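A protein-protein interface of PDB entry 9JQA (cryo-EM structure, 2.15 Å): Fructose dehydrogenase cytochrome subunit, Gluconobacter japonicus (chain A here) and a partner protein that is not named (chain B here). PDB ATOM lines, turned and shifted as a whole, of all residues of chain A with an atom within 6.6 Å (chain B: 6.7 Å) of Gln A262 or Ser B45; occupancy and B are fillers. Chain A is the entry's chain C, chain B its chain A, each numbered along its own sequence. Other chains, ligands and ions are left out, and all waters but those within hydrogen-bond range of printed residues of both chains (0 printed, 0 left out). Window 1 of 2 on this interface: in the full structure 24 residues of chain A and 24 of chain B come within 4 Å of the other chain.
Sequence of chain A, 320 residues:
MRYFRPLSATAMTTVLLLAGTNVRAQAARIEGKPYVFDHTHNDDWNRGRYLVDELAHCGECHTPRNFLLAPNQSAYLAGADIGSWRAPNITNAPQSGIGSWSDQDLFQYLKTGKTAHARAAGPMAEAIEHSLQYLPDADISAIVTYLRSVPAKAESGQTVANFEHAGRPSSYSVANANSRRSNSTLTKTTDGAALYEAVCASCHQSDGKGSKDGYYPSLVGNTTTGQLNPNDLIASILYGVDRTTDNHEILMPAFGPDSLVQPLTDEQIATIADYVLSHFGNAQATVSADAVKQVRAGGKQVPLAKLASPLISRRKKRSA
NH1 of Arg B44 lies within hydrogen-bond range of O of Cys B226 (2.8 Å). NE2 of Gln B46 sits at hydrogen-bond distance from OE1 of Glu B49, 3.2 Å away. The side-chain amide oxygen of Asn B50 is in hydrogen-bond range of the side-chain amide nitrogen of Gln B46 (2.8 Å). The side-chain amide nitrogen (NE2) of Gln A268 lies within hydrogen-bond range of the backbone carbonyl oxygen (O) of Leu A186, at 3.5 Å. The side-chain hydroxyl of Ser A259 lies within hydrogen-bond range of the backbone NH of Val A261, 3.3 Å away. The backbone NH of Gln A262 lies within hydrogen-bond range of the side-chain hydroxyl of Ser A259, at 3.1 Å.
The side-chain carboxylate of Asp B43 is in hydrogen-bond range of the backbone NH of Leu A186, 3.2 Å away. The side-chain amide nitrogen of Gln A262 is in hydrogen-bond range of the side-chain carboxylate of Asp B43, 3.4 Å away. O of Val A261 lies within hydrogen-bond range of NE of Arg B44 (2.9 Å). The backbone NH of Arg B44 sits at hydrogen-bond distance from the side-chain amide oxygen of Gln A262 (2.9 Å). The backbone NH (N) of Ser B45 sits at hydrogen-bond distance from the side-chain amide oxygen (OE1) of Gln A262 (3.0 Å). The guanidinium group (NH1) of Arg B52 sits at hydrogen-bond distance from the backbone carbonyl oxygen (O) of Glu A197 (2.5 Å).
Of the 16 printed residues of chain A, 7 touch a printed residue of chain B. Of the 15 printed residues of chain B, 6 touch a printed residue of chain A. Among the printed residues, 12 pairs touch across the chains.
CD1 of Leu A186 touches CB of Ser B45 (3.6 Å). Gln B46 touches Leu A186 (OE1 to CD2, 3.5 Å). Ala A198 touches Ser B45 (O to OG, 3.5 Å). Ala A198 touches Arg B52 (CA to NH1, 3.7 Å). Ser B45 touches Val A199. CD2 of Leu A260 touches CG2 of Ile B239, at 3.7 Å.
Of chain A, only Leu A186 (3.6 Å), Ala A198 (3.5 Å), Val A199 (3.2 Å) and Gln A262 (3.0 Å) come within 4 Å of Ser B45. Printed residues of chain B within 4 Å of Glu A197: Arg B52 (2.5 Å). Of the printed residues of chain B, Leu A186 touches Asp B43, Ser B45 and Gln B46. Of the printed residues of chain A, Asp B43 touches Leu A186 and Gln A262. Of the printed residues of chain A, Ile B239 touches Leu A260 (3.7 Å). Of the printed residues of chain A, Arg B52 touches Glu A197 (2.5 Å) and Ala A198 (3.7 Å). The nearest residue of chain B that does not touch Gln A262 is Gln B46 (4.7 Å).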
ATOM      1  N   LEU A 186       7.314 -15.966  26.350  1.00  0.00           N
ATOM      2  CA  LEU A 186       8.125 -14.899  26.920  1.00  0.00           C
ATOM      3  C   LEU A 186       7.402 -13.563  26.981  1.00  0.00           C
ATOM      4  O   LEU A 186       8.042 -12.553  27.290  1.00  0.00           O
ATOM      5  CB  LEU A 186       9.412 -14.724  26.113  1.00  0.00           C
ATOM      6  CG  LEU A 186      10.499 -15.792  26.174  1.00  0.00           C
ATOM      7  CD1 LEU A 186      11.463 -15.581  25.028  1.00  0.00           C
ATOM      8  CD2 LEU A 186      11.231 -15.747  27.500  1.00  0.00           C
ATOM      9  N   LEU A 195      15.298 -11.652  30.158  1.00  0.00           N
ATOM     10  CA  LEU A 195      15.306 -12.021  28.748  1.00  0.00           C
ATOM     11  C   LEU A 195      16.690 -12.468  28.301  1.00  0.00           C
ATOM     12  O   LEU A 195      16.826 -13.463  27.581  1.00  0.00           O
ATOM     13  CB  LEU A 195      14.820 -10.852  27.895  1.00  0.00           C
ATOM     14  CG  LEU A 195      13.310 -10.695  27.738  1.00  0.00           C
ATOM     15  CD1 LEU A 195      12.988  -9.365  27.088  1.00  0.00           C
ATOM     16  CD2 LEU A 195      12.736 -11.840  26.928  1.00  0.00           C
ATOM     17  N   GLU A 197      18.982 -13.776  30.201  1.00  0.00           N
ATOM     18  CA  GLU A 197      19.268 -15.064  30.819  1.00  0.00           C
ATOM     19  C   GLU A 197      18.536 -16.197  30.112  1.00  0.00           C
ATOM     20  O   GLU A 197      19.109 -17.269  29.892  1.00  0.00           O
ATOM     21  CB  GLU A 197      18.902 -15.032  32.300  1.00  0.00           C
ATOM     22  CG  GLU A 197      19.424 -16.221  33.076  1.00  0.00           C
ATOM     23  CD  GLU A 197      20.847 -16.028  33.548  1.00  0.00           C
ATOM     24  OE1 GLU A 197      21.364 -14.898  33.436  1.00  0.00           O
ATOM     25  OE2 GLU A 197      21.450 -17.003  34.035  1.00  0.00           O
ATOM     26  N   ALA A 198      17.272 -15.983  29.753  1.00  0.00           N
ATOM     27  CA  ALA A 198      16.481 -17.055  29.158  1.00  0.00           C
ATOM     28  C   ALA A 198      16.915 -17.338  27.726  1.00  0.00           C
ATOM     29  O   ALA A 198      17.093 -18.497  27.338  1.00  0.00           O
ATOM     30  CB  ALA A 198      14.997 -16.699  29.212  1.00  0.00           C
ATOM     31  N   VAL A 199      17.095 -16.291  26.928  1.00  0.00           N
ATOM     32  CA  VAL A 199      17.364 -16.475  25.509  1.00  0.00           C
ATOM     33  C   VAL A 199      18.850 -16.642  25.226  1.00  0.00           C
ATOM     34  O   VAL A 199      19.226 -17.317  24.263  1.00  0.00           O
ATOM     35  CB  VAL A 199      16.793 -15.291  24.710  1.00  0.00           C
ATOM     36  CG1 VAL A 199      16.884 -15.554  23.219  1.00  0.00           C
ATOM     37  CG2 VAL A 199      15.360 -15.011  25.115  1.00  0.00           C
ATOM     38  N   CYS A 200      19.704 -16.067  26.062  1.00  0.00           N
ATOM     39  CA  CYS A 200      21.046 -15.733  25.625  1.00  0.00           C
ATOM     40  C   CYS A 200      22.151 -16.156  26.582  1.00  0.00           C
ATOM     41  O   CYS A 200      23.313 -16.158  26.170  1.00  0.00           O
ATOM     42  CB  CYS A 200      21.112 -14.214  25.398  1.00  0.00           C
ATOM     43  SG  CYS A 200      22.544 -13.610  24.570  1.00  0.00           S
ATOM     44  N   ALA A 254      20.119 -17.094  14.518  1.00  0.00           N
ATOM     45  CA  ALA A 254      19.360 -15.858  14.418  1.00  0.00           C
ATOM     46  C   ALA A 254      18.256 -15.830  15.466  1.00  0.00           C
ATOM     47  O   ALA A 254      17.717 -16.866  15.862  1.00  0.00           O
ATOM     48  CB  ALA A 254      18.762 -15.708  13.023  1.00  0.00           C
ATOM     49  N   PHE A 255      17.920 -14.623  15.922  1.00  0.00           N
ATOM     50  CA  PHE A 255      16.863 -14.447  16.911  1.00  0.00           C
ATOM     51  C   PHE A 255      15.820 -13.434  16.457  1.00  0.00           C
ATOM     52  O   PHE A 255      15.092 -12.890  17.290  1.00  0.00           O
ATOM     53  CB  PHE A 255      17.445 -14.038  18.265  1.00  0.00           C
ATOM     54  CG  PHE A 255      18.171 -15.144  18.965  1.00  0.00           C
ATOM     55  CD1 PHE A 255      17.475 -16.186  19.544  1.00  0.00           C
ATOM     56  CD2 PHE A 255      19.551 -15.149  19.033  1.00  0.00           C
ATOM     57  CE1 PHE A 255      18.139 -17.207  20.181  1.00  0.00           C
ATOM     58  CE2 PHE A 255      20.218 -16.169  19.671  1.00  0.00           C
ATOM     59  CZ  PHE A 255      19.511 -17.198  20.245  1.00  0.00           C
ATOM     60  N   GLY A 256      15.726 -13.174  15.158  1.00  0.00           N
ATOM     61  CA  GLY A 256      14.727 -12.275  14.633  1.00  0.00           C
ATOM     62  C   GLY A 256      13.389 -12.963  14.470  1.00  0.00           C
ATOM     63  O   GLY A 256      13.155 -14.048  15.009  1.00  0.00           O
ATOM     64  N   SER A 259      13.459 -16.575  13.279  1.00  0.00           N
ATOM     65  CA  SER A 259      14.305 -17.466  14.059  1.00  0.00           C
ATOM     66  C   SER A 259      13.662 -18.836  14.220  1.00  0.00           C
ATOM     67  O   SER A 259      12.450 -18.955  14.413  1.00  0.00           O
ATOM     68  CB  SER A 259      14.577 -16.861  15.433  1.00  0.00           C
ATOM     69  OG  SER A 259      15.425 -17.695  16.199  1.00  0.00           O
ATOM     70  N   LEU A 260      14.488 -19.875  14.139  1.00  0.00           N
ATOM     71  CA  LEU A 260      14.050 -21.224  14.464  1.00  0.00           C
ATOM     72  C   LEU A 260      14.225 -21.546  15.939  1.00  0.00           C
ATOM     73  O   LEU A 260      13.470 -22.358  16.484  1.00  0.00           O
ATOM     74  CB  LEU A 260      14.824 -22.250  13.634  1.00  0.00           C
ATOM     75  CG  LEU A 260      14.400 -22.459  12.182  1.00  0.00           C
ATOM     76  CD1 LEU A 260      15.198 -23.593  11.571  1.00  0.00           C
ATOM     77  CD2 LEU A 260      12.916 -22.741  12.095  1.00  0.00           C
ATOM     78  N   VAL A 261      15.199 -20.920  16.596  1.00  0.00           N
ATOM     79  CA  VAL A 261      15.489 -21.236  17.988  1.00  0.00           C
ATOM     80  C   VAL A 261      14.559 -20.473  18.921  1.00  0.00           C
ATOM     81  O   VAL A 261      13.887 -21.065  19.772  1.00  0.00           O
ATOM     82  CB  VAL A 261      16.968 -20.940  18.296  1.00  0.00           C
ATOM     83  CG1 VAL A 261      17.244 -21.104  19.774  1.00  0.00           C
ATOM     84  CG2 VAL A 261      17.860 -21.848  17.476  1.00  0.00           C
ATOM     85  N   GLN A 262      14.511 -19.157  18.783  1.00  0.00           N
ATOM     86  CA  GLN A 262      13.657 -18.334  19.626  1.00  0.00           C
ATOM     87  C   GLN A 262      13.354 -17.014  18.936  1.00  0.00           C
ATOM     88  O   GLN A 262      14.157 -16.076  19.015  1.00  0.00           O
ATOM     89  CB  GLN A 262      14.313 -18.083  20.983  1.00  0.00           C
ATOM     90  CG  GLN A 262      13.487 -17.210  21.907  1.00  0.00           C
ATOM     91  CD  GLN A 262      12.079 -17.731  22.087  1.00  0.00           C
ATOM     92  OE1 GLN A 262      11.869 -18.777  22.692  1.00  0.00           O
ATOM     93  NE2 GLN A 262      11.107 -17.002  21.559  1.00  0.00           N
ATOM     94  N   PRO A 263      12.229 -16.905  18.234  1.00  0.00           N
ATOM     95  CA  PRO A 263      11.855 -15.615  17.647  1.00  0.00           C
ATOM     96  C   PRO A 263      11.673 -14.558  18.724  1.00  0.00           C
ATOM     97  O   PRO A 263      11.117 -14.822  19.791  1.00  0.00           O
ATOM     98  CB  PRO A 263      10.537 -15.920  16.928  1.00  0.00           C
ATOM     99  CG  PRO A 263      10.519 -17.394  16.763  1.00  0.00           C
ATOM    100  CD  PRO A 263      11.246 -17.955  17.933  1.00  0.00           C
ATOM    101  N   LEU A 264      12.142 -13.352  18.433  1.00  0.00           N
ATOM    102  CA  LEU A 264      12.043 -12.237  19.360  1.00  0.00           C
ATOM    103  C   LEU A 264      11.449 -11.037  18.645  1.00  0.00           C
ATOM    104  O   LEU A 264      11.778 -10.768  17.487  1.00  0.00           O
ATOM    105  CB  LEU A 264      13.408 -11.869  19.945  1.00  0.00           C
ATOM    106  CG  LEU A 264      14.126 -12.931  20.774  1.00  0.00           C
ATOM    107  CD1 LEU A 264      15.539 -12.483  21.081  1.00  0.00           C
ATOM    108  CD2 LEU A 264      13.365 -13.216  22.051  1.00  0.00           C
ATOM    109  N   GLN A 268      11.529  -6.951  22.424  1.00  0.00           N
ATOM    110  CA  GLN A 268      12.358  -7.884  23.180  1.00  0.00           C
ATOM    111  C   GLN A 268      13.823  -7.778  22.780  1.00  0.00           C
ATOM    112  O   GLN A 268      14.710  -7.818  23.640  1.00  0.00           O
ATOM    113  CB  GLN A 268      11.850  -9.311  22.984  1.00  0.00           C
ATOM    114  CG  GLN A 268      10.486  -9.562  23.589  1.00  0.00           C
ATOM    115  CD  GLN A 268       9.943 -10.929  23.245  1.00  0.00           C
ATOM    116  OE1 GLN A 268      10.204 -11.459  22.170  1.00  0.00           O
ATOM    117  NE2 GLN A 268       9.178 -11.505  24.159  1.00  0.00           N
ATOM    118  N   ARG B  42       4.423 -22.226  22.284  1.00  0.00           N
ATOM    119  CA  ARG B  42       5.421 -22.266  23.340  1.00  0.00           C
ATOM    120  C   ARG B  42       6.719 -21.653  22.842  1.00  0.00           C
ATOM    121  O   ARG B  42       7.112 -21.856  21.691  1.00  0.00           O
ATOM    122  CB  ARG B  42       5.663 -23.702  23.818  1.00  0.00           C
ATOM    123  CG  ARG B  42       4.391 -24.475  24.104  1.00  0.00           C
ATOM    124  CD  ARG B  42       4.603 -25.516  25.182  1.00  0.00           C
ATOM    125  NE  ARG B  42       3.383 -26.256  25.479  1.00  0.00           N
ATOM    126  CZ  ARG B  42       2.667 -26.107  26.584  1.00  0.00           C
ATOM    127  NH1 ARG B  42       3.012 -25.241  27.520  1.00  0.00           N
ATOM    128  NH2 ARG B  42       1.578 -26.848  26.755  1.00  0.00           N
ATOM    129  N   ASP B  43       7.373 -20.896  23.715  1.00  0.00           N
ATOM    130  CA  ASP B  43       8.665 -20.291  23.425  1.00  0.00           C
ATOM    131  C   ASP B  43       9.756 -21.099  24.110  1.00  0.00           C
ATOM    132  O   ASP B  43       9.626 -21.449  25.286  1.00  0.00           O
ATOM    133  CB  ASP B  43       8.711 -18.838  23.895  1.00  0.00           C
ATOM    134  CG  ASP B  43       8.098 -17.884  22.896  1.00  0.00           C
ATOM    135  OD1 ASP B  43       7.959 -18.259  21.714  1.00  0.00           O
ATOM    136  OD2 ASP B  43       7.755 -16.751  23.290  1.00  0.00           O
ATOM    137  N   ARG B  44      10.827 -21.391  23.371  1.00  0.00           N
ATOM    138  CA  ARG B  44      11.899 -22.217  23.913  1.00  0.00           C
ATOM    139  C   ARG B  44      12.530 -21.575  25.140  1.00  0.00           C
ATOM    140  O   ARG B  44      12.788 -22.252  26.140  1.00  0.00           O
ATOM    141  CB  ARG B  44      12.954 -22.469  22.838  1.00  0.00           C
ATOM    142  CG  ARG B  44      14.319 -22.850  23.375  1.00  0.00           C
ATOM    143  CD  ARG B  44      15.318 -22.993  22.247  1.00  0.00           C
ATOM    144  NE  ARG B  44      14.696 -23.560  21.058  1.00  0.00           N
ATOM    145  CZ  ARG B  44      14.617 -24.857  20.801  1.00  0.00           C
ATOM    146  NH1 ARG B  44      15.140 -25.757  21.616  1.00  0.00           N
ATOM    147  NH2 ARG B  44      13.996 -25.261  19.700  1.00  0.00           N
ATOM    148  N   SER B  45      12.775 -20.265  25.087  1.00  0.00           N
ATOM    149  CA  SER B  45      13.462 -19.600  26.188  1.00  0.00           C
ATOM    150  C   SER B  45      12.604 -19.568  27.446  1.00  0.00           C
ATOM    151  O   SER B  45      13.128 -19.663  28.560  1.00  0.00           O
ATOM    152  CB  SER B  45      13.865 -18.191  25.773  1.00  0.00           C
ATOM    153  OG  SER B  45      14.783 -18.238  24.700  1.00  0.00           O
ATOM    154  N   GLN B  46      11.288 -19.427  27.294  1.00  0.00           N
ATOM    155  CA  GLN B  46      10.419 -19.482  28.465  1.00  0.00           C
ATOM    156  C   GLN B  46      10.439 -20.865  29.100  1.00  0.00           C
ATOM    157  O   GLN B  46      10.442 -20.987  30.326  1.00  0.00           O
ATOM    158  CB  GLN B  46       8.995 -19.081  28.095  1.00  0.00           C
ATOM    159  CG  GLN B  46       8.087 -18.921  29.298  1.00  0.00           C
ATOM    160  CD  GLN B  46       8.652 -17.969  30.329  1.00  0.00           C
ATOM    161  OE1 GLN B  46       9.028 -16.844  30.010  1.00  0.00           O
ATOM    162  NE2 GLN B  46       8.716 -18.416  31.574  1.00  0.00           N
ATOM    163  N   ILE B  47      10.453 -21.918  28.282  1.00  0.00           N
ATOM    164  CA  ILE B  47      10.556 -23.269  28.821  1.00  0.00           C
ATOM    165  C   ILE B  47      11.895 -23.459  29.520  1.00  0.00           C
ATOM    166  O   ILE B  47      11.986 -24.136  30.548  1.00  0.00           O
ATOM    167  CB  ILE B  47      10.345 -24.313  27.709  1.00  0.00           C
ATOM    168  CG1 ILE B  47       9.042 -24.046  26.958  1.00  0.00           C
ATOM    169  CG2 ILE B  47      10.339 -25.706  28.294  1.00  0.00           C
ATOM    170  CD1 ILE B  47       7.823 -23.964  27.846  1.00  0.00           C
ATOM    171  N   VAL B  48      12.954 -22.864  28.971  1.00  0.00           N
ATOM    172  CA  VAL B  48      14.265 -22.934  29.609  1.00  0.00           C
ATOM    173  C   VAL B  48      14.231 -22.258  30.972  1.00  0.00           C
ATOM    174  O   VAL B  48      14.753 -22.789  31.959  1.00  0.00           O
ATOM    175  CB  VAL B  48      15.331 -22.308  28.695  1.00  0.00           C
ATOM    176  CG1 VAL B  48      16.648 -22.174  29.428  1.00  0.00           C
ATOM    177  CG2 VAL B  48      15.496 -23.143  27.456  1.00  0.00           C
ATOM    178  N   GLU B  49      13.620 -21.076  31.046  1.00  0.00           N
ATOM    179  CA  GLU B  49      13.503 -20.385  32.326  1.00  0.00           C
ATOM    180  C   GLU B  49      12.670 -21.191  33.313  1.00  0.00           C
ATOM    181  O   GLU B  49      12.996 -21.256  34.502  1.00  0.00           O
ATOM    182  CB  GLU B  49      12.898 -18.998  32.126  1.00  0.00           C
ATOM    183  CG  GLU B  49      13.052 -18.092  33.331  1.00  0.00           C
ATOM    184  CD  GLU B  49      12.107 -16.913  33.303  1.00  0.00           C
ATOM    185  OE1 GLU B  49      10.898 -17.111  33.535  1.00  0.00           O
ATOM    186  OE2 GLU B  49      12.573 -15.784  33.049  1.00  0.00           O
ATOM    187  N   ASN B  50      11.586 -21.806  32.837  1.00  0.00           N
ATOM    188  CA  ASN B  50      10.751 -22.622  33.710  1.00  0.00           C
ATOM    189  C   ASN B  50      11.522 -23.818  34.249  1.00  0.00           C
ATOM    190  O   ASN B  50      11.392 -24.168  35.426  1.00  0.00           O
ATOM    191  CB  ASN B  50       9.502 -23.085  32.964  1.00  0.00           C
ATOM    192  CG  ASN B  50       8.572 -21.946  32.620  1.00  0.00           C
ATOM    193  OD1 ASN B  50       8.752 -20.823  33.082  1.00  0.00           O
ATOM    194  ND2 ASN B  50       7.572 -22.231  31.801  1.00  0.00           N
ATOM    195  N   ARG B  52      14.813 -23.999  34.599  1.00  0.00           N
ATOM    196  CA  ARG B  52      15.836 -23.503  35.512  1.00  0.00           C
ATOM    197  C   ARG B  52      15.250 -23.212  36.885  1.00  0.00           C
ATOM    198  O   ARG B  52      15.900 -23.447  37.908  1.00  0.00           O
ATOM    199  CB  ARG B  52      16.495 -22.253  34.936  1.00  0.00           C
ATOM    200  CG  ARG B  52      17.485 -22.534  33.829  1.00  0.00           C
ATOM    201  CD  ARG B  52      17.885 -21.264  33.119  1.00  0.00           C
ATOM    202  NE  ARG B  52      18.917 -21.500  32.119  1.00  0.00           N
ATOM    203  CZ  ARG B  52      19.237 -20.644  31.160  1.00  0.00           C
ATOM    204  NH1 ARG B  52      18.630 -19.475  31.049  1.00  0.00           N
ATOM    205  NH2 ARG B  52      20.185 -20.970  30.290  1.00  0.00           N
ATOM    206  N   TRP B 109       9.112 -31.257  21.666  1.00  0.00           N
ATOM    207  CA  TRP B 109       9.673 -30.154  22.434  1.00  0.00           C
ATOM    208  C   TRP B 109      10.662 -30.643  23.484  1.00  0.00           C
ATOM    209  O   TRP B 109      11.650 -29.958  23.767  1.00  0.00           O
ATOM    210  CB  TRP B 109       8.554 -29.364  23.107  1.00  0.00           C
ATOM    211  CG  TRP B 109       8.186 -28.094  22.415  1.00  0.00           C
ATOM    212  CD1 TRP B 109       6.969 -27.770  21.903  1.00  0.00           C
ATOM    213  CD2 TRP B 109       9.036 -26.969  22.172  1.00  0.00           C
ATOM    214  NE1 TRP B 109       7.005 -26.516  21.351  1.00  0.00           N
ATOM    215  CE2 TRP B 109       8.266 -26.002  21.502  1.00  0.00           C
ATOM    216  CE3 TRP B 109      10.375 -26.686  22.453  1.00  0.00           C
ATOM    217  CZ2 TRP B 109       8.786 -24.775  21.111  1.00  0.00           C
ATOM    218  CZ3 TRP B 109      10.889 -25.471  22.060  1.00  0.00           C
ATOM    219  CH2 TRP B 109      10.097 -24.529  21.398  1.00  0.00           C
ATOM    220  N   ILE B 225      14.445 -29.576  27.662  1.00  0.00           N
ATOM    221  CA  ILE B 225      14.505 -28.456  26.728  1.00  0.00           C
ATOM    222  C   ILE B 225      15.947 -28.087  26.409  1.00  0.00           C
ATOM    223  O   ILE B 225      16.774 -27.910  27.308  1.00  0.00           O
ATOM    224  CB  ILE B 225      13.726 -27.239  27.272  1.00  0.00           C
ATOM    225  CG1 ILE B 225      13.780 -26.081  26.277  1.00  0.00           C
ATOM    226  CG2 ILE B 225      14.222 -26.831  28.650  1.00  0.00           C
ATOM    227  CD1 ILE B 225      13.008 -26.342  25.016  1.00  0.00           C
ATOM    228  N   CYS B 226      16.252 -27.961  25.120  1.00  0.00           N
ATOM    229  CA  CYS B 226      17.546 -27.455  24.694  1.00  0.00           C
ATOM    230  C   CYS B 226      17.496 -25.936  24.658  1.00  0.00           C
ATOM    231  O   CYS B 226      16.664 -25.374  23.935  1.00  0.00           O
ATOM    232  CB  CYS B 226      17.917 -27.994  23.326  1.00  0.00           C
ATOM    233  SG  CYS B 226      19.460 -27.330  22.673  1.00  0.00           S
ATOM    234  N   PRO B 227      18.345 -25.237  25.413  1.00  0.00           N
ATOM    235  CA  PRO B 227      18.258 -23.771  25.445  1.00  0.00           C
ATOM    236  C   PRO B 227      18.659 -23.095  24.150  1.00  0.00           C
ATOM    237  O   PRO B 227      18.268 -21.944  23.930  1.00  0.00           O
ATOM    238  CB  PRO B 227      19.209 -23.391  26.586  1.00  0.00           C
ATOM    239  CG  PRO B 227      20.156 -24.522  26.673  1.00  0.00           C
ATOM    240  CD  PRO B 227      19.391 -25.751  26.308  1.00  0.00           C
ATOM    241  N   ILE B 239       7.333 -23.939  12.151  1.00  0.00           N
ATOM    242  CA  ILE B 239       7.772 -22.596  11.785  1.00  0.00           C
ATOM    243  C   ILE B 239       8.023 -22.510  10.287  1.00  0.00           C
ATOM    244  O   ILE B 239       7.615 -21.549   9.625  1.00  0.00           O
ATOM    245  CB  ILE B 239       9.024 -22.206  12.591  1.00  0.00           C
ATOM    246  CG1 ILE B 239       8.673 -22.002  14.063  1.00  0.00           C
ATOM    247  CG2 ILE B 239       9.658 -20.954  12.021  1.00  0.00           C
ATOM    248  CD1 ILE B 239       9.866 -22.064  14.980  1.00  0.00           C
